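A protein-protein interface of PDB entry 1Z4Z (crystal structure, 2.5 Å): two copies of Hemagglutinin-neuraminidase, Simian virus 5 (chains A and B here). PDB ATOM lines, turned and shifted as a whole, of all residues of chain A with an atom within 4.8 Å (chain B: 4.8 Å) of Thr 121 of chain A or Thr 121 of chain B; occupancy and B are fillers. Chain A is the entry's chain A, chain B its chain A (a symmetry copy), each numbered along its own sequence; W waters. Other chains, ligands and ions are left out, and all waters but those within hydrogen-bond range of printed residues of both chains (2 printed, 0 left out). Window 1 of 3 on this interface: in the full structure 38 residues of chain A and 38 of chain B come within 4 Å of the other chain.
The backbone NH of Met 115 of chain A lies within hydrogen-bond range of the side-chain hydroxyl of Thr 123 of chain B, 3.0 Å away.
O of Thr 121 of chain A lies within hydrogen-bond range of N of Ser 117 of chain B (2.8 Å).
The backbone NH (N) of Met 115 of chain B lies within hydrogen-bond range of the side-chain hydroxyl (OG1) of Thr 123 of chain A (3.0 Å).
The backbone carbonyl oxygen (O) of Thr 121 of chain B is in hydrogen-bond range of the backbone NH (N) of Ser 117 of chain A (2.8 Å).
The backbone NH (N) of Ile 119 of chain B lies within hydrogen-bond range of the side-chain hydroxyl (OG) of Ser 117 of chain B.
OG of Ser 117 of chain A lies within hydrogen-bond range of N of Ile 119 of chain A, 3.3 Å away.
Met 115 of chain A touches Thr 121 of chain B.
Pro 120 of chain B touches Pro 116 of chain A (CB to CB, 3.97 Å).
Thr 121 of chain B touches Pro 116 of chain A (O to C, 3.7 Å).
Pro 120 of chain B touches Ser 117 of chain A (CB to O, 3.2 Å).
Ser 117 of chain B touches Pro 120 of chain A.
Thr 121 of chain A touches Met 115 of chain B.
C of Pro 116 of chain B touches O of Thr 121 of chain A, at 3.7 Å.
CG2 of Thr 121 of chain A touches NE2 of Gln 521 of chain B (3.3 Å).
Thr 121 of chain B touches Gln 521 of chain A (CG2 to NE2, 3.3 Å).
Gln 521 of chain B touches Gln 521 of chain A.
Printed residues of chain B within 4 Å of Ser 117 of chain A: Pro 120 (3.2 Å) and Thr 121 (2.8 Å).
Thr 121 of chain A touches just these residues of chain B: Met 115, Pro 116, Ser 117, Thr 121 and Gln 521.
Ala 122 of chain A touches none of the printed residues of chain B.
Of the printed residues of chain B, Thr 123 of chain A touches Met 115.
Leu 517 of chain A touches none of the printed residues of chain B.
Of the printed residues of chain B, Gln 521 of chain A touches Thr 121 and Gln 521.
Of the printed residues of chain A, Pro 120 of chain B touches Pro 116 (3.97 Å) and Ser 117 (3.2 Å).
Of the printed residues of chain A, Thr 121 of chain B touches Met 115, Pro 116, Ser 117, Thr 121 and Gln 521.
Printed residues of chain A within 4 Å of Thr 123 of chain B: Met 115 (3.0 Å).
The nearest printed residue of chain B that does not touch Thr 121 of chain A is Ile 119 of chain B (5.5 Å).
The nearest printed residue of chain A that does not touch Thr 121 of chain B is Ile 119 of chain A (5.5 Å).
Printed residues of chain A that touch a printed residue of chain B: Met 115, Pro 116, Ser 117, Pro 120, Thr 121, Thr 123 and Gln 521.
Hydrophobic or aromatic side chains of chain A within 4 Å of the printed part of chain B: Met 115, Pro 116 and Pro 120.
Of the 10 printed residues of chain B, 7 touch a printed residue of chain A.
Hydrophobic or aromatic side chains of chain B that line the printed part of chain A: Met 115, Pro 116 and Pro 120.
Among the printed residues, no Asp or Glu carboxylate lies within 4 Å of a Lys or Arg side-chain nitrogen of the other chain.
Met 115 of chain A touches Thr 121 of chain B, and with the chains exchanged Thr 121 of chain A touches Met 115 of chain B.
Met 115 of chain A touches Thr 123 of chain B, and with the chains exchanged Thr 123 of chain A touches Met 115 of chain B.
Pro 116 of chain A touches Thr 121 of chain B, and with the chains exchanged Thr 121 of chain A touches Pro 116 of chain B.
Gln 521 of chain B touches its own counterpart, Gln 521 of chain A.
Of the 16 pairs that touch across the chains among the printed residues, 16 have their exchanged pair printed and touching as well.
Water W2 bridges the backbone carbonyl oxygen of Ile 119 of chain A (2.8 Å) and the backbone NH of Thr 121 of chain B (2.9 Å).
Water W1 bridges O of Ile 119 of chain B (2.8 Å) and N of Thr 121 of chain A (2.9 Å).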
ATOM      1  N   MET A 115     -17.028  -3.653  26.826  1.00  0.00           N
ATOM      2  CA  MET A 115     -17.183  -5.078  26.571  1.00  0.00           C
ATOM      3  C   MET A 115     -16.149  -5.464  25.526  1.00  0.00           C
ATOM      4  O   MET A 115     -15.681  -4.617  24.772  1.00  0.00           O
ATOM      5  CB  MET A 115     -18.585  -5.387  26.040  1.00  0.00           C
ATOM      6  CG  MET A 115     -18.860  -4.827  24.664  1.00  0.00           C
ATOM      7  SD  MET A 115     -20.465  -5.316  24.012  1.00  0.00           S
ATOM      8  CE  MET A 115     -20.355  -4.606  22.348  1.00  0.00           C
ATOM      9  N   PRO A 116     -15.750  -6.747  25.485  1.00  0.00           N
ATOM     10  CA  PRO A 116     -14.758  -7.147  24.480  1.00  0.00           C
ATOM     11  C   PRO A 116     -15.386  -6.968  23.101  1.00  0.00           C
ATOM     12  O   PRO A 116     -16.453  -7.512  22.828  1.00  0.00           O
ATOM     13  CB  PRO A 116     -14.504  -8.615  24.804  1.00  0.00           C
ATOM     14  CG  PRO A 116     -14.779  -8.691  26.284  1.00  0.00           C
ATOM     15  CD  PRO A 116     -16.024  -7.848  26.424  1.00  0.00           C
ATOM     16  N   SER A 117     -14.736  -6.195  22.241  1.00  0.00           N
ATOM     17  CA  SER A 117     -15.264  -5.963  20.911  1.00  0.00           C
ATOM     18  C   SER A 117     -15.290  -7.254  20.107  1.00  0.00           C
ATOM     19  O   SER A 117     -14.345  -8.041  20.154  1.00  0.00           O
ATOM     20  CB  SER A 117     -14.420  -4.924  20.173  1.00  0.00           C
ATOM     21  OG  SER A 117     -14.965  -4.661  18.885  1.00  0.00           O
ATOM     22  N   ILE A 119     -15.767  -7.076  16.832  1.00  0.00           N
ATOM     23  CA  ILE A 119     -15.422  -6.633  15.482  1.00  0.00           C
ATOM     24  C   ILE A 119     -13.903  -6.547  15.387  1.00  0.00           C
ATOM     25  O   ILE A 119     -13.275  -5.745  16.074  1.00  0.00           O
ATOM     26  CB  ILE A 119     -16.040  -5.259  15.175  1.00  0.00           C
ATOM     27  CG1 ILE A 119     -17.561  -5.339  15.322  1.00  0.00           C
ATOM     28  CG2 ILE A 119     -15.683  -4.829  13.778  1.00  0.00           C
ATOM     29  CD1 ILE A 119     -18.284  -4.041  15.069  1.00  0.00           C
ATOM     30  N   PRO A 120     -13.293  -7.381  14.532  1.00  0.00           N
ATOM     31  CA  PRO A 120     -11.838  -7.409  14.357  1.00  0.00           C
ATOM     32  C   PRO A 120     -11.197  -6.141  13.815  1.00  0.00           C
ATOM     33  O   PRO A 120     -11.739  -5.455  12.950  1.00  0.00           O
ATOM     34  CB  PRO A 120     -11.626  -8.608  13.437  1.00  0.00           C
ATOM     35  CG  PRO A 120     -12.843  -8.565  12.575  1.00  0.00           C
ATOM     36  CD  PRO A 120     -13.950  -8.289  13.574  1.00  0.00           C
ATOM     37  N   THR A 121     -10.012  -5.871  14.340  1.00  0.00           N
ATOM     38  CA  THR A 121      -9.193  -4.718  14.005  1.00  0.00           C
ATOM     39  C   THR A 121      -8.128  -5.076  12.958  1.00  0.00           C
ATOM     40  O   THR A 121      -7.760  -6.241  12.807  1.00  0.00           O
ATOM     41  CB  THR A 121      -8.517  -4.214  15.307  1.00  0.00           C
ATOM     42  OG1 THR A 121      -9.441  -3.387  16.022  1.00  0.00           O
ATOM     43  CG2 THR A 121      -7.248  -3.450  15.025  1.00  0.00           C
ATOM     44  N   ALA A 122      -7.644  -4.074  12.229  1.00  0.00           N
ATOM     45  CA  ALA A 122      -6.601  -4.288  11.231  1.00  0.00           C
ATOM     46  C   ALA A 122      -5.280  -4.412  11.993  1.00  0.00           C
ATOM     47  O   ALA A 122      -5.190  -3.994  13.147  1.00  0.00           O
ATOM     48  CB  ALA A 122      -6.546  -3.115  10.268  1.00  0.00           C
ATOM     49  N   THR A 123      -4.258  -4.988  11.361  1.00  0.00           N
ATOM     50  CA  THR A 123      -2.968  -5.153  12.025  1.00  0.00           C
ATOM     51  C   THR A 123      -1.819  -4.426  11.321  1.00  0.00           C
ATOM     52  O   THR A 123      -0.648  -4.721  11.559  1.00  0.00           O
ATOM     53  CB  THR A 123      -2.610  -6.650  12.168  1.00  0.00           C
ATOM     54  OG1 THR A 123      -2.623  -7.277  10.879  1.00  0.00           O
ATOM     55  CG2 THR A 123      -3.611  -7.347  13.067  1.00  0.00           C
ATOM     56  N   LEU A 517      -3.606   1.723  14.317  1.00  0.00           N
ATOM     57  CA  LEU A 517      -3.747   0.579  13.418  1.00  0.00           C
ATOM     58  C   LEU A 517      -4.888   0.756  12.427  1.00  0.00           C
ATOM     59  O   LEU A 517      -6.012   1.062  12.815  1.00  0.00           O
ATOM     60  CB  LEU A 517      -3.986  -0.703  14.223  1.00  0.00           C
ATOM     61  CG  LEU A 517      -2.794  -1.399  14.882  1.00  0.00           C
ATOM     62  CD1 LEU A 517      -1.841  -1.903  13.813  1.00  0.00           C
ATOM     63  CD2 LEU A 517      -2.098  -0.441  15.821  1.00  0.00           C
ATOM     64  N   GLN A 521     -11.249   1.937  12.381  1.00  0.00           N
ATOM     65  CA  GLN A 521     -11.431   0.941  13.415  1.00  0.00           C
ATOM     66  C   GLN A 521     -12.936   0.954  13.603  1.00  0.00           C
ATOM     67  O   GLN A 521     -13.497   1.950  14.052  1.00  0.00           O
ATOM     68  CB  GLN A 521     -10.743   1.329  14.729  1.00  0.00           C
ATOM     69  CG  GLN A 521     -10.733   0.181  15.740  1.00  0.00           C
ATOM     70  CD  GLN A 521     -10.106   0.538  17.082  1.00  0.00           C
ATOM     71  OE1 GLN A 521      -9.092   1.233  17.140  1.00  0.00           O
ATOM     72  NE2 GLN A 521     -10.697   0.041  18.168  1.00  0.00           N
ATOM     73  N   MET B 115      -4.162  -8.706   8.685  1.00  0.00           N
ATOM     74  CA  MET B 115      -5.118  -9.791   8.852  1.00  0.00           C
ATOM     75  C   MET B 115      -6.126  -9.348   9.899  1.00  0.00           C
ATOM     76  O   MET B 115      -5.834  -8.479  10.715  1.00  0.00           O
ATOM     77  CB  MET B 115      -4.417 -11.067   9.327  1.00  0.00           C
ATOM     78  CG  MET B 115      -3.854 -10.976  10.727  1.00  0.00           C
ATOM     79  SD  MET B 115      -3.152 -12.529  11.306  1.00  0.00           S
ATOM     80  CE  MET B 115      -2.744 -12.069  13.013  1.00  0.00           C
ATOM     81  N   PRO B 116      -7.344  -9.916   9.875  1.00  0.00           N
ATOM     82  CA  PRO B 116      -8.333  -9.510  10.880  1.00  0.00           C
ATOM     83  C   PRO B 116      -7.815  -9.936  12.251  1.00  0.00           C
ATOM     84  O   PRO B 116      -7.506 -11.106  12.463  1.00  0.00           O
ATOM     85  CB  PRO B 116      -9.581 -10.288  10.478  1.00  0.00           C
ATOM     86  CG  PRO B 116      -9.414 -10.455   8.989  1.00  0.00           C
ATOM     87  CD  PRO B 116      -7.950 -10.801   8.865  1.00  0.00           C
ATOM     88  N   SER B 117      -7.703  -8.987  13.171  1.00  0.00           N
ATOM     89  CA  SER B 117      -7.211  -9.300  14.499  1.00  0.00           C
ATOM     90  C   SER B 117      -8.169 -10.233  15.224  1.00  0.00           C
ATOM     91  O   SER B 117      -9.385 -10.060  15.155  1.00  0.00           O
ATOM     92  CB  SER B 117      -7.030  -8.023  15.318  1.00  0.00           C
ATOM     93  OG  SER B 117      -6.502  -8.325  16.605  1.00  0.00           O
ATOM     94  N   ILE B 119      -7.802 -10.659  18.490  1.00  0.00           N
ATOM     95  CA  ILE B 119      -7.741 -10.187  19.873  1.00  0.00           C
ATOM     96  C   ILE B 119      -8.702  -9.011  20.012  1.00  0.00           C
ATOM     97  O   ILE B 119      -8.514  -7.969  19.390  1.00  0.00           O
ATOM     98  CB  ILE B 119      -6.318  -9.740  20.244  1.00  0.00           C
ATOM     99  CG1 ILE B 119      -5.350 -10.910  20.053  1.00  0.00           C
ATOM    100  CG2 ILE B 119      -6.277  -9.270  21.672  1.00  0.00           C
ATOM    101  CD1 ILE B 119      -3.910 -10.589  20.363  1.00  0.00           C
ATOM    102  N   PRO B 120      -9.752  -9.170  20.832  1.00  0.00           N
ATOM    103  CA  PRO B 120     -10.756  -8.124  21.043  1.00  0.00           C
ATOM    104  C   PRO B 120     -10.264  -6.831  21.675  1.00  0.00           C
ATOM    105  O   PRO B 120      -9.415  -6.822  22.565  1.00  0.00           O
ATOM    106  CB  PRO B 120     -11.809  -8.826  21.896  1.00  0.00           C
ATOM    107  CG  PRO B 120     -10.981  -9.748  22.727  1.00  0.00           C
ATOM    108  CD  PRO B 120     -10.006 -10.322  21.717  1.00  0.00           C
ATOM    109  N   THR B 121     -10.848  -5.743  21.199  1.00  0.00           N
ATOM    110  CA  THR B 121     -10.555  -4.384  21.622  1.00  0.00           C
ATOM    111  C   THR B 121     -11.564  -3.898  22.673  1.00  0.00           C
ATOM    112  O   THR B 121     -12.676  -4.417  22.766  1.00  0.00           O
ATOM    113  CB  THR B 121     -10.604  -3.469  20.370  1.00  0.00           C
ATOM    114  OG1 THR B 121      -9.351  -3.556  19.681  1.00  0.00           O
ATOM    115  CG2 THR B 121     -10.900  -2.036  20.729  1.00  0.00           C
ATOM    116  N   ALA B 122     -11.167  -2.911  23.473  1.00  0.00           N
ATOM    117  CA  ALA B 122     -12.053  -2.343  24.484  1.00  0.00           C
ATOM    118  C   ALA B 122     -13.015  -1.404  23.750  1.00  0.00           C
ATOM    119  O   ALA B 122     -12.736  -0.989  22.625  1.00  0.00           O
ATOM    120  CB  ALA B 122     -11.249  -1.572  25.515  1.00  0.00           C
ATOM    121  N   THR B 123     -14.144  -1.072  24.373  1.00  0.00           N
ATOM    122  CA  THR B 123     -15.117  -0.190  23.734  1.00  0.00           C
ATOM    123  C   THR B 123     -15.370   1.106  24.509  1.00  0.00           C
ATOM    124  O   THR B 123     -16.371   1.787  24.286  1.00  0.00           O
ATOM    125  CB  THR B 123     -16.461  -0.921  23.512  1.00  0.00           C
ATOM    126  OG1 THR B 123     -16.950  -1.428  24.762  1.00  0.00           O
ATOM    127  CG2 THR B 123     -16.279  -2.076  22.548  1.00  0.00           C
ATOM    128  N   LEU B 517      -9.544   4.086  21.837  1.00  0.00           N
ATOM    129  CA  LEU B 517     -10.319   3.161  22.662  1.00  0.00           C
ATOM    130  C   LEU B 517      -9.446   2.377  23.631  1.00  0.00           C
ATOM    131  O   LEU B 517      -8.454   1.775  23.233  1.00  0.00           O
ATOM    132  CB  LEU B 517     -11.084   2.172  21.777  1.00  0.00           C
ATOM    133  CG  LEU B 517     -12.383   2.625  21.109  1.00  0.00           C
ATOM    134  CD1 LEU B 517     -13.425   2.928  22.171  1.00  0.00           C
ATOM    135  CD2 LEU B 517     -12.120   3.837  20.246  1.00  0.00           C
ATOM    136  N   GLN B 521      -4.294  -1.535  23.582  1.00  0.00           N
ATOM    137  CA  GLN B 521      -4.881  -2.278  22.486  1.00  0.00           C
ATOM    138  C   GLN B 521      -3.854  -3.371  22.259  1.00  0.00           C
ATOM    139  O   GLN B 521      -2.729  -3.091  21.856  1.00  0.00           O
ATOM    140  CB  GLN B 521      -5.023  -1.431  21.216  1.00  0.00           C
ATOM    141  CG  GLN B 521      -5.851  -2.134  20.139  1.00  0.00           C
ATOM    142  CD  GLN B 521      -5.975  -1.352  18.838  1.00  0.00           C
ATOM    143  OE1 GLN B 521      -6.142  -0.133  18.847  1.00  0.00           O
ATOM    144  NE2 GLN B 521      -5.916  -2.059  17.709  1.00  0.00           N
HETATM  145  O   HOH W   1      -9.648  -6.820  17.085  1.00  0.00           O
HETATM  146  O   HOH W   2     -11.723  -5.949  18.413  1.00  0.00           O
